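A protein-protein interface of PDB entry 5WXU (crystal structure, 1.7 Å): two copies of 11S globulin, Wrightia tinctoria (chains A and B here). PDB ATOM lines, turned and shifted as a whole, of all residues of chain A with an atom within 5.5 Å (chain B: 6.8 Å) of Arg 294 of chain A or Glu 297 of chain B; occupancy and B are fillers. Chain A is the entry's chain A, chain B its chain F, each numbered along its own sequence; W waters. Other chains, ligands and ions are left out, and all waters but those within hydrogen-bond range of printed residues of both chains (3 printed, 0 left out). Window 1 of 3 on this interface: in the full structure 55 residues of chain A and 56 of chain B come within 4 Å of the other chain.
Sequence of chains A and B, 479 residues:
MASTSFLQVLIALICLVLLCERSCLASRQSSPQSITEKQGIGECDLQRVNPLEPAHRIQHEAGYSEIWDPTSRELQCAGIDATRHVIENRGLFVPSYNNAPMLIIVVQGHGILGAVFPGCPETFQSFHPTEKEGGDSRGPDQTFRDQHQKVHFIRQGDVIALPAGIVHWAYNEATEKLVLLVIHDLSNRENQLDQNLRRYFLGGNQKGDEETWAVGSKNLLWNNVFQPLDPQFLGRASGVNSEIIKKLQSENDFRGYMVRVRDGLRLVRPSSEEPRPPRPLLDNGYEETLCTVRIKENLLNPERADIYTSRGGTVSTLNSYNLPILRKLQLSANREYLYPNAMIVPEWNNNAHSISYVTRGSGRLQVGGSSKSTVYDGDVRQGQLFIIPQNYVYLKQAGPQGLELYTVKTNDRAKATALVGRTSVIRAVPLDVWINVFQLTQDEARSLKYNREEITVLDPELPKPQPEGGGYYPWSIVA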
ATOM      1  N   THR A 292      10.677 -31.399  -7.575  1.00  0.00           N
ATOM      2  CA  THR A 292      10.701 -29.949  -7.827  1.00  0.00           C
ATOM      3  C   THR A 292      11.662 -29.489  -8.902  1.00  0.00           C
ATOM      4  O   THR A 292      11.921 -28.304  -8.977  1.00  0.00           O
ATOM      5  CB  THR A 292      11.097 -29.102  -6.557  1.00  0.00           C
ATOM      6  OG1 THR A 292      12.503 -29.292  -6.106  1.00  0.00           O
ATOM      7  CG2 THR A 292      10.086 -29.352  -5.490  1.00  0.00           C
ATOM      8  N   VAL A 293      12.242 -30.428  -9.635  1.00  0.00           N
ATOM      9  CA  VAL A 293      13.368 -30.120 -10.514  1.00  0.00           C
ATOM     10  C   VAL A 293      12.971 -28.902 -11.390  1.00  0.00           C
ATOM     11  O   VAL A 293      11.840 -28.833 -11.942  1.00  0.00           O
ATOM     12  CB  VAL A 293      13.820 -31.373 -11.285  1.00  0.00           C
ATOM     13  CG1 VAL A 293      12.686 -31.917 -12.160  1.00  0.00           C
ATOM     14  CG2 VAL A 293      15.008 -31.122 -12.211  1.00  0.00           C
ATOM     15  N   ARG A 294      13.884 -27.945 -11.597  1.00  0.00           N
ATOM     16  CA  ARG A 294      13.551 -26.801 -12.465  1.00  0.00           C
ATOM     17  C   ARG A 294      13.636 -27.237 -13.949  1.00  0.00           C
ATOM     18  O   ARG A 294      14.547 -27.916 -14.338  1.00  0.00           O
ATOM     19  CB  ARG A 294      14.514 -25.642 -12.237  1.00  0.00           C
ATOM     20  CG  ARG A 294      14.098 -24.371 -12.952  1.00  0.00           C
ATOM     21  CD  ARG A 294      14.615 -23.117 -12.274  1.00  0.00           C
ATOM     22  NE  ARG A 294      16.042 -23.245 -12.165  1.00  0.00           N
ATOM     23  CZ  ARG A 294      16.967 -22.838 -13.063  1.00  0.00           C
ATOM     24  NH1 ARG A 294      16.686 -22.306 -14.212  1.00  0.00           N
ATOM     25  NH2 ARG A 294      18.231 -23.004 -12.799  1.00  0.00           N
ATOM     26  N   ILE A 295      12.679 -26.810 -14.754  1.00  0.00           N
ATOM     27  CA  ILE A 295      12.558 -27.244 -16.155  1.00  0.00           C
ATOM     28  C   ILE A 295      12.861 -26.124 -17.156  1.00  0.00           C
ATOM     29  O   ILE A 295      12.874 -26.361 -18.345  1.00  0.00           O
ATOM     30  CB  ILE A 295      11.155 -27.822 -16.430  1.00  0.00           C
ATOM     31  CG1 ILE A 295      10.787 -28.941 -15.422  1.00  0.00           C
ATOM     32  CG2 ILE A 295      11.032 -28.422 -17.802  1.00  0.00           C
ATOM     33  CD1 ILE A 295      11.665 -30.166 -15.509  1.00  0.00           C
ATOM     34  N   LYS A 296      13.054 -24.897 -16.721  1.00  0.00           N
ATOM     35  CA  LYS A 296      13.235 -23.869 -17.695  1.00  0.00           C
ATOM     36  C   LYS A 296      14.037 -22.741 -17.148  1.00  0.00           C
ATOM     37  O   LYS A 296      14.099 -22.565 -15.912  1.00  0.00           O
ATOM     38  CB  LYS A 296      11.910 -23.349 -18.155  1.00  0.00           C
ATOM     39  CG  LYS A 296      11.076 -22.655 -17.127  1.00  0.00           C
ATOM     40  CD  LYS A 296       9.824 -22.181 -17.775  1.00  0.00           C
ATOM     41  CE  LYS A 296       8.914 -21.483 -16.809  1.00  0.00           C
ATOM     42  NZ  LYS A 296       9.316 -20.058 -16.777  1.00  0.00           N
ATOM     43  N   GLU A 297      14.631 -21.982 -18.051  1.00  0.00           N
ATOM     44  CA  GLU A 297      15.267 -20.725 -17.723  1.00  0.00           C
ATOM     45  C   GLU A 297      14.950 -19.694 -18.795  1.00  0.00           C
ATOM     46  O   GLU A 297      14.906 -20.077 -19.999  1.00  0.00           O
ATOM     47  CB  GLU A 297      16.726 -20.998 -17.696  1.00  0.00           C
ATOM     48  CG  GLU A 297      17.502 -19.842 -17.191  1.00  0.00           C
ATOM     49  CD  GLU A 297      18.729 -20.179 -16.389  1.00  0.00           C
ATOM     50  OE1 GLU A 297      18.769 -21.152 -15.601  1.00  0.00           O
ATOM     51  OE2 GLU A 297      19.630 -19.389 -16.556  1.00  0.00           O
ATOM     52  N   ASN A 322      23.936 -23.825 -15.074  1.00  0.00           N
ATOM     53  CA  ASN A 322      22.761 -22.920 -14.974  1.00  0.00           C
ATOM     54  C   ASN A 322      21.440 -23.688 -14.629  1.00  0.00           C
ATOM     55  O   ASN A 322      20.656 -23.233 -13.739  1.00  0.00           O
ATOM     56  CB  ASN A 322      22.580 -22.094 -16.298  1.00  0.00           C
ATOM     57  CG  ASN A 322      23.880 -21.467 -16.857  1.00  0.00           C
ATOM     58  OD1 ASN A 322      24.211 -21.502 -18.096  1.00  0.00           O
ATOM     59  ND2 ASN A 322      24.662 -20.898 -15.938  1.00  0.00           N
ATOM     60  N   LEU A 323      21.196 -24.835 -15.303  1.00  0.00           N
ATOM     61  CA  LEU A 323      19.955 -25.608 -15.220  1.00  0.00           C
ATOM     62  C   LEU A 323      20.345 -27.049 -15.039  1.00  0.00           C
ATOM     63  O   LEU A 323      20.843 -27.667 -15.963  1.00  0.00           O
ATOM     64  CB  LEU A 323      19.140 -25.344 -16.505  1.00  0.00           C
ATOM     65  CG  LEU A 323      17.838 -26.041 -16.656  1.00  0.00           C
ATOM     66  CD1 LEU A 323      16.888 -25.693 -15.485  1.00  0.00           C
ATOM     67  CD2 LEU A 323      17.155 -25.700 -17.997  1.00  0.00           C
ATOM     68  N   PRO A 324      20.163 -27.615 -13.827  1.00  0.00           N
ATOM     69  CA  PRO A 324      20.771 -28.880 -13.498  1.00  0.00           C
ATOM     70  C   PRO A 324      20.309 -30.026 -14.400  1.00  0.00           C
ATOM     71  O   PRO A 324      21.074 -30.948 -14.669  1.00  0.00           O
ATOM     72  CB  PRO A 324      20.249 -29.131 -12.068  1.00  0.00           C
ATOM     73  CG  PRO A 324      20.082 -27.788 -11.514  1.00  0.00           C
ATOM     74  CD  PRO A 324      19.611 -26.957 -12.622  1.00  0.00           C
ATOM     75  N   ILE A 325      19.060 -29.974 -14.855  1.00  0.00           N
ATOM     76  CA  ILE A 325      18.437 -31.126 -15.614  1.00  0.00           C
ATOM     77  C   ILE A 325      19.170 -31.330 -16.967  1.00  0.00           C
ATOM     78  O   ILE A 325      19.204 -32.401 -17.537  1.00  0.00           O
ATOM     79  CB  ILE A 325      16.925 -30.961 -15.829  1.00  0.00           C
ATOM     80  CG1 ILE A 325      16.313 -32.338 -16.241  1.00  0.00           C
ATOM     81  CG2 ILE A 325      16.601 -29.788 -16.749  1.00  0.00           C
ATOM     82  CD1 ILE A 325      14.831 -32.288 -16.353  1.00  0.00           C
ATOM     83  N   GLY B 157      13.409 -10.970  -3.179  1.00  0.00           N
ATOM     84  CA  GLY B 157      13.092 -12.362  -3.318  1.00  0.00           C
ATOM     85  C   GLY B 157      14.230 -13.226  -3.831  1.00  0.00           C
ATOM     86  O   GLY B 157      14.092 -14.437  -3.849  1.00  0.00           O
ATOM     87  N   ASP B 158      15.326 -12.601  -4.335  1.00  0.00           N
ATOM     88  CA  ASP B 158      16.469 -13.319  -4.797  1.00  0.00           C
ATOM     89  C   ASP B 158      17.175 -13.964  -3.647  1.00  0.00           C
ATOM     90  O   ASP B 158      17.315 -13.378  -2.531  1.00  0.00           O
ATOM     91  CB  ASP B 158      17.442 -12.401  -5.550  1.00  0.00           C
ATOM     92  CG  ASP B 158      17.091 -12.148  -6.952  1.00  0.00           C
ATOM     93  OD1 ASP B 158      16.206 -12.809  -7.499  1.00  0.00           O
ATOM     94  OD2 ASP B 158      17.777 -11.251  -7.537  1.00  0.00           O
ATOM     95  N   VAL B 159      17.557 -15.216  -3.828  1.00  0.00           N
ATOM     96  CA  VAL B 159      18.473 -15.882  -2.930  1.00  0.00           C
ATOM     97  C   VAL B 159      19.783 -16.133  -3.723  1.00  0.00           C
ATOM     98  O   VAL B 159      19.784 -16.763  -4.777  1.00  0.00           O
ATOM     99  CB  VAL B 159      17.904 -17.230  -2.457  1.00  0.00           C
ATOM    100  CG1 VAL B 159      18.928 -17.932  -1.580  1.00  0.00           C
ATOM    101  CG2 VAL B 159      16.631 -17.029  -1.711  1.00  0.00           C
ATOM    102  N   ILE B 160      20.893 -15.643  -3.215  1.00  0.00           N
ATOM    103  CA  ILE B 160      22.164 -15.710  -3.899  1.00  0.00           C
ATOM    104  C   ILE B 160      23.108 -16.594  -3.086  1.00  0.00           C
ATOM    105  O   ILE B 160      23.189 -16.458  -1.904  1.00  0.00           O
ATOM    106  CB  ILE B 160      22.763 -14.272  -3.983  1.00  0.00           C
ATOM    107  CG1 ILE B 160      21.843 -13.270  -4.670  1.00  0.00           C
ATOM    108  CG2 ILE B 160      24.096 -14.260  -4.666  1.00  0.00           C
ATOM    109  CD1 ILE B 160      21.801 -11.935  -3.898  1.00  0.00           C
ATOM    110  N   ALA B 161      23.845 -17.462  -3.765  1.00  0.00           N
ATOM    111  CA  ALA B 161      24.706 -18.460  -3.207  1.00  0.00           C
ATOM    112  C   ALA B 161      26.122 -18.122  -3.607  1.00  0.00           C
ATOM    113  O   ALA B 161      26.431 -18.160  -4.783  1.00  0.00           O
ATOM    114  CB  ALA B 161      24.297 -19.831  -3.734  1.00  0.00           C
ATOM    115  N   ARG B 294      25.370 -20.169 -12.552  1.00  0.00           N
ATOM    116  CA  ARG B 294      24.259 -19.477 -11.967  1.00  0.00           C
ATOM    117  C   ARG B 294      24.516 -19.379 -10.483  1.00  0.00           C
ATOM    118  O   ARG B 294      24.919 -20.300  -9.776  1.00  0.00           O
ATOM    119  CB  ARG B 294      22.916 -20.146 -12.218  1.00  0.00           C
ATOM    120  CG  ARG B 294      21.730 -19.342 -11.721  1.00  0.00           C
ATOM    121  CD  ARG B 294      20.444 -19.589 -12.495  1.00  0.00           C
ATOM    122  NE  ARG B 294      19.452 -18.600 -12.088  1.00  0.00           N
ATOM    123  CZ  ARG B 294      18.854 -17.682 -12.853  1.00  0.00           C
ATOM    124  NH1 ARG B 294      19.071 -17.559 -14.180  1.00  0.00           N
ATOM    125  NH2 ARG B 294      17.983 -16.876 -12.257  1.00  0.00           N
ATOM    126  N   ILE B 295      24.262 -17.795  -9.900  1.00  0.00           N
ATOM    127  CA  ILE B 295      24.485 -17.613  -8.479  1.00  0.00           C
ATOM    128  C   ILE B 295      23.175 -17.375  -7.736  1.00  0.00           C
ATOM    129  O   ILE B 295      23.189 -17.220  -6.518  1.00  0.00           O
ATOM    130  CB  ILE B 295      25.488 -16.460  -8.287  1.00  0.00           C
ATOM    131  CG1 ILE B 295      26.749 -16.737  -9.066  1.00  0.00           C
ATOM    132  CG2 ILE B 295      25.917 -16.300  -6.852  1.00  0.00           C
ATOM    133  CD1 ILE B 295      27.568 -17.877  -8.500  1.00  0.00           C
ATOM    134  N   LYS B 296      22.062 -17.248  -8.450  1.00  0.00           N
ATOM    135  CA  LYS B 296      20.869 -16.854  -7.783  1.00  0.00           C
ATOM    136  C   LYS B 296      19.596 -17.318  -8.412  1.00  0.00           C
ATOM    137  O   LYS B 296      19.555 -17.665  -9.600  1.00  0.00           O
ATOM    138  CB  LYS B 296      20.823 -15.382  -7.605  1.00  0.00           C
ATOM    139  CG  LYS B 296      20.430 -14.618  -8.806  1.00  0.00           C
ATOM    140  CD  LYS B 296      20.538 -13.139  -8.508  1.00  0.00           C
ATOM    141  CE  LYS B 296      20.332 -12.354  -9.760  1.00  0.00           C
ATOM    142  NZ  LYS B 296      18.899 -12.315 -10.158  1.00  0.00           N
ATOM    143  N   GLU B 297      18.536 -17.221  -7.626  1.00  0.00           N
ATOM    144  CA  GLU B 297      17.200 -17.607  -8.079  1.00  0.00           C
ATOM    145  C   GLU B 297      16.209 -16.763  -7.255  1.00  0.00           C
ATOM    146  O   GLU B 297      16.389 -16.631  -6.021  1.00  0.00           O
ATOM    147  CB  GLU B 297      16.940 -19.125  -7.832  1.00  0.00           C
ATOM    148  CG  GLU B 297      15.708 -19.556  -8.627  1.00  0.00           C
ATOM    149  CD  GLU B 297      15.682 -21.003  -8.996  1.00  0.00           C
ATOM    150  OE1 GLU B 297      16.725 -21.534  -9.438  1.00  0.00           O
ATOM    151  OE2 GLU B 297      14.607 -21.599  -8.807  1.00  0.00           O
ATOM    152  N   ASN B 298      15.143 -16.296  -7.892  1.00  0.00           N
ATOM    153  CA  ASN B 298      14.116 -15.579  -7.176  1.00  0.00           C
ATOM    154  C   ASN B 298      13.044 -16.491  -6.659  1.00  0.00           C
ATOM    155  O   ASN B 298      12.550 -17.361  -7.386  1.00  0.00           O
ATOM    156  CB  ASN B 298      13.520 -14.538  -8.068  1.00  0.00           C
ATOM    157  CG  ASN B 298      12.728 -13.533  -7.307  1.00  0.00           C
ATOM    158  OD1 ASN B 298      11.527 -13.719  -7.087  1.00  0.00           O
ATOM    159  ND2 ASN B 298      13.371 -12.410  -6.961  1.00  0.00           N
ATOM    160  N   LEU B 299      12.578 -16.263  -5.432  1.00  0.00           N
ATOM    161  CA  LEU B 299      11.581 -17.094  -4.866  1.00  0.00           C
ATOM    162  C   LEU B 299      10.227 -16.398  -4.649  1.00  0.00           C
ATOM    163  O   LEU B 299       9.346 -17.005  -4.056  1.00  0.00           O
ATOM    164  CB  LEU B 299      12.055 -17.678  -3.548  1.00  0.00           C
ATOM    165  CG  LEU B 299      13.268 -18.595  -3.561  1.00  0.00           C
ATOM    166  CD1 LEU B 299      13.565 -19.249  -2.243  1.00  0.00           C
ATOM    167  CD2 LEU B 299      13.072 -19.688  -4.607  1.00  0.00           C
ATOM    168  N   LEU B 300      10.116 -15.140  -5.049  1.00  0.00           N
ATOM    169  CA  LEU B 300       8.985 -14.310  -4.624  1.00  0.00           C
ATOM    170  C   LEU B 300       7.658 -14.485  -5.309  1.00  0.00           C
ATOM    171  O   LEU B 300       6.628 -14.286  -4.669  1.00  0.00           O
ATOM    172  CB  LEU B 300       9.356 -12.859  -4.774  1.00  0.00           C
ATOM    173  CG  LEU B 300       8.425 -11.840  -4.142  1.00  0.00           C
ATOM    174  CD1 LEU B 300       7.873 -12.244  -2.776  1.00  0.00           C
ATOM    175  CD2 LEU B 300       9.149 -10.542  -4.074  1.00  0.00           C
ATOM    176  N   ARG B 304       6.092 -19.462  -8.797  1.00  0.00           N
ATOM    177  CA  ARG B 304       7.333 -20.320  -8.563  1.00  0.00           C
ATOM    178  C   ARG B 304       7.134 -21.347  -7.416  1.00  0.00           C
ATOM    179  O   ARG B 304       8.022 -22.087  -6.979  1.00  0.00           O
ATOM    180  CB  ARG B 304       8.514 -19.363  -8.254  1.00  0.00           C
ATOM    181  CG  ARG B 304       9.801 -19.866  -7.569  1.00  0.00           C
ATOM    182  CD  ARG B 304      10.541 -20.699  -8.606  1.00  0.00           C
ATOM    183  NE  ARG B 304      11.765 -21.305  -8.086  1.00  0.00           N
ATOM    184  CZ  ARG B 304      11.788 -22.269  -7.151  1.00  0.00           C
ATOM    185  NH1 ARG B 304      10.676 -22.759  -6.635  1.00  0.00           N
ATOM    186  NH2 ARG B 304      12.948 -22.756  -6.716  1.00  0.00           N
ATOM    187  N   THR B 317      10.819 -23.986  -3.010  1.00  0.00           N
ATOM    188  CA  THR B 317      12.039 -24.639  -2.502  1.00  0.00           C
ATOM    189  C   THR B 317      13.189 -24.282  -3.444  1.00  0.00           C
ATOM    190  O   THR B 317      12.973 -24.131  -4.632  1.00  0.00           O
ATOM    191  CB  THR B 317      11.913 -26.172  -2.530  1.00  0.00           C
ATOM    192  OG1 THR B 317      11.747 -26.603  -3.908  1.00  0.00           O
ATOM    193  CG2 THR B 317      10.830 -26.552  -1.693  1.00  0.00           C
ATOM    194  N   LEU B 318      14.396 -24.146  -2.897  1.00  0.00           N
ATOM    195  CA  LEU B 318      15.584 -23.829  -3.650  1.00  0.00           C
ATOM    196  C   LEU B 318      16.685 -24.807  -3.225  1.00  0.00           C
ATOM    197  O   LEU B 318      17.217 -24.702  -2.167  1.00  0.00           O
ATOM    198  CB  LEU B 318      16.020 -22.392  -3.465  1.00  0.00           C
ATOM    199  CG  LEU B 318      17.175 -22.002  -4.348  1.00  0.00           C
ATOM    200  CD1 LEU B 318      16.748 -22.028  -5.825  1.00  0.00           C
ATOM    201  CD2 LEU B 318      17.651 -20.610  -3.975  1.00  0.00           C
ATOM    202  N   ASN B 319      16.993 -25.792  -4.084  1.00  0.00           N
ATOM    203  CA  ASN B 319      18.007 -26.726  -3.793  1.00  0.00           C
ATOM    204  C   ASN B 319      18.747 -27.095  -5.094  1.00  0.00           C
ATOM    205  O   ASN B 319      18.566 -26.389  -6.104  1.00  0.00           O
ATOM    206  CB  ASN B 319      17.440 -27.996  -3.130  1.00  0.00           C
ATOM    207  CG  ASN B 319      16.364 -28.634  -3.937  1.00  0.00           C
ATOM    208  OD1 ASN B 319      16.462 -28.901  -5.166  1.00  0.00           O
ATOM    209  ND2 ASN B 319      15.255 -28.894  -3.224  1.00  0.00           N
ATOM    210  N   TYR B 321      18.633 -29.346  -7.245  1.00  0.00           N
ATOM    211  CA  TYR B 321      17.835 -29.691  -8.431  1.00  0.00           C
ATOM    212  C   TYR B 321      17.359 -28.470  -9.204  1.00  0.00           C
ATOM    213  O   TYR B 321      16.779 -28.580 -10.320  1.00  0.00           O
ATOM    214  CB  TYR B 321      16.631 -30.569  -8.057  1.00  0.00           C
ATOM    215  CG  TYR B 321      16.994 -31.964  -7.629  1.00  0.00           C
ATOM    216  CD1 TYR B 321      17.570 -32.832  -8.530  1.00  0.00           C
ATOM    217  CD2 TYR B 321      16.812 -32.391  -6.334  1.00  0.00           C
ATOM    218  CE1 TYR B 321      17.939 -34.099  -8.158  1.00  0.00           C
ATOM    219  CE2 TYR B 321      17.133 -33.682  -5.962  1.00  0.00           C
ATOM    220  CZ  TYR B 321      17.699 -34.525  -6.885  1.00  0.00           C
ATOM    221  OH  TYR B 321      18.108 -35.806  -6.586  1.00  0.00           O
ATOM    222  N   ASN B 322      17.522 -27.262  -8.599  1.00  0.00           N
ATOM    223  CA  ASN B 322      17.111 -25.979  -9.154  1.00  0.00           C
ATOM    224  C   ASN B 322      18.365 -25.095  -9.511  1.00  0.00           C
ATOM    225  O   ASN B 322      18.415 -24.498 -10.592  1.00  0.00           O
ATOM    226  CB  ASN B 322      16.183 -25.190  -8.156  1.00  0.00           C
ATOM    227  CG  ASN B 322      15.046 -26.053  -7.503  1.00  0.00           C
ATOM    228  OD1 ASN B 322      14.804 -26.099  -6.228  1.00  0.00           O
ATOM    229  ND2 ASN B 322      14.317 -26.734  -8.365  1.00  0.00           N
ATOM    230  N   LEU B 323      19.317 -24.990  -8.576  1.00  0.00           N
ATOM    231  CA  LEU B 323      20.448 -24.091  -8.613  1.00  0.00           C
ATOM    232  C   LEU B 323      21.693 -24.926  -8.400  1.00  0.00           C
ATOM    233  O   LEU B 323      21.980 -25.439  -7.302  1.00  0.00           O
ATOM    234  CB  LEU B 323      20.301 -23.006  -7.578  1.00  0.00           C
ATOM    235  CG  LEU B 323      21.420 -21.969  -7.516  1.00  0.00           C
ATOM    236  CD1 LEU B 323      21.576 -21.277  -8.821  1.00  0.00           C
ATOM    237  CD2 LEU B 323      21.107 -20.975  -6.432  1.00  0.00           C
ATOM    238  N   PRO B 324      22.447 -25.163  -9.469  1.00  0.00           N
ATOM    239  CA  PRO B 324      23.431 -26.231  -9.276  1.00  0.00           C
ATOM    240  C   PRO B 324      24.558 -26.002  -8.264  1.00  0.00           C
ATOM    241  O   PRO B 324      25.108 -26.944  -7.731  1.00  0.00           O
ATOM    242  CB  PRO B 324      24.090 -26.380 -10.661  1.00  0.00           C
ATOM    243  CG  PRO B 324      23.148 -25.756 -11.604  1.00  0.00           C
ATOM    244  CD  PRO B 324      22.222 -24.820 -10.869  1.00  0.00           C
HETATM  245  O   HOH W   1      11.189 -25.540  -8.430  1.00  0.00           O
HETATM  246  O   HOH W   2      22.280 -18.204 -15.183  1.00  0.00           O
HETATM  247  O   HOH W   3      17.022 -28.687 -13.191  1.00  0.00           O
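ND2 of Asn 322 of chain B sits at hydrogen-bond distance from O of Thr 292 of chain A, 2.9 Å away. The side-chain carboxylate (OE1) of Glu 297 of chain B is in salt-bridge range of the guanidinium group (NE) of Arg 294 of chain A (3.3 Å). N of Arg 294 of chain A is in hydrogen-bond range of O of Tyr 321 of chain B. The guanidinium group (NH2) of Arg 294 of chain A sits at hydrogen-bond distance from the backbone carbonyl oxygen (O) of Asn 322 of chain B (2.7 Å). The side-chain carboxylate (OE2) of Glu 297 of chain A lies within salt-bridge range of the guanidinium group (NH1) of Arg 294 of chain B (3.1 Å).
The guanidinium group of Arg 294 of chain A sits at hydrogen-bond distance from the backbone carbonyl oxygen of Lys 296 of chain A (3.1 Å). O of Asn 322 of chain A sits at hydrogen-bond distance from NH2 of Arg 294 of chain A, 2.6 Å away. The backbone NH (N) of Val 159 of chain B is in hydrogen-bond range of the backbone carbonyl oxygen (O) of Glu 297 of chain B (2.9 Å). The backbone carbonyl oxygen of Lys 296 of chain B lies within hydrogen-bond range of the guanidinium group of Arg 294 of chain B (2.7 Å). OD1 of Asn 319 of chain B is in hydrogen-bond range of N of Tyr 321 of chain B. The backbone NH of Asn 319 of chain B is in hydrogen-bond range of the side-chain amide oxygen of Asn 322 of chain B.
OG1 of Thr 292 of chain A touches OG1 of Thr 317 of chain B (3.6 Å). O of Tyr 321 of chain B touches CG2 of Val 293 of chain A, at 3.6 Å. Asn 322 of chain B touches Val 293 of chain A. N of Arg 294 of chain B touches ND2 of Asn 322 of chain A, at 3.5 Å. O of Asn 322 of chain A touches CD of Pro 324 of chain B (3.6 Å). CG of Pro 324 of chain A touches O of Tyr 321 of chain B, 3.6 Å away. O of Asn 322 of chain B touches CD of Pro 324 of chain A (3.4 Å). Pro 324 of chain A touches Pro 324 of chain B (CG to CG, 3.7 Å).
Of the printed residues of chain B, Asn 322 of chain A touches Arg 294 and Pro 324. Printed residues of chain A within 4 Å of Glu 297 of chain B: Arg 294 (3.3 Å). Of the printed residues of chain A, Thr 317 of chain B touches Thr 292 (3.6 Å). Of the printed residues of chain A, Tyr 321 of chain B touches Val 293 (3.6 Å), Arg 294 (3.2 Å) and Pro 324 (3.6 Å). Printed residues of chain A within 4 Å of Pro 324 of chain B: Asn 322 (3.6 Å) and Pro 324 (3.7 Å). The nearest printed residue of chain A that does not touch Glu 297 of chain B is Asn 322 of chain A (6.1 Å).
Of the 20 printed residues of chain B, 6 touch a printed residue of chain A. Printed residues of chain B that touch a printed residue of chain A: Arg 294, Glu 297, Thr 317, Tyr 321, Asn 322 and Pro 324. Hydrophobic or aromatic side chains of chain B that line the printed part of chain A: Pro 324. Among the printed residues, Asp or Glu carboxylates within 4 Å of a Lys or Arg side-chain nitrogen of the other chain: Arg 294 of chain A with Glu 297 of chain B (3.3 Å) and Glu 297 of chain A with Arg 294 of chain B (3.1 Å).
Arg 294 of chain A touches Glu 297 of chain B, and with the chains exchanged Glu 297 of chain A touches Arg 294 of chain B. Arg 294 of chain A touches Asn 322 of chain B, and with the chains exchanged Asn 322 of chain A touches Arg 294 of chain B. Asn 322 of chain A touches Pro 324 of chain B, and with the chains exchanged Pro 324 of chain A touches Asn 322 of chain B. Pro 324 of chain B touches its own counterpart, Pro 324 of chain A. Positions printed for both chains: 294, 295, 296, 297, 322, 323 and 324. Of the 13 pairs that touch across the chains among the printed residues, 7 have their exchanged pair printed and touching as well.
Water W3 lies within hydrogen-bond range of the backbone carbonyl oxygen of Arg 294 of chain A (2.8 Å), the backbone carbonyl oxygen of Tyr 321 of chain B (2.9 Å) and the backbone NH of Ile 325 of chain A (2.9 Å). Water W1 lies within hydrogen-bond range of O of Thr 292 of chain A (2.9 Å), ND2 of Asn 322 of chain B (3.3 Å) and NH1 of Arg 304 of chain B (3.3 Å). Water W2 lies within hydrogen-bond range of OE2 of Glu 297 of chain A and NH1 of Arg 294 of chain B.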
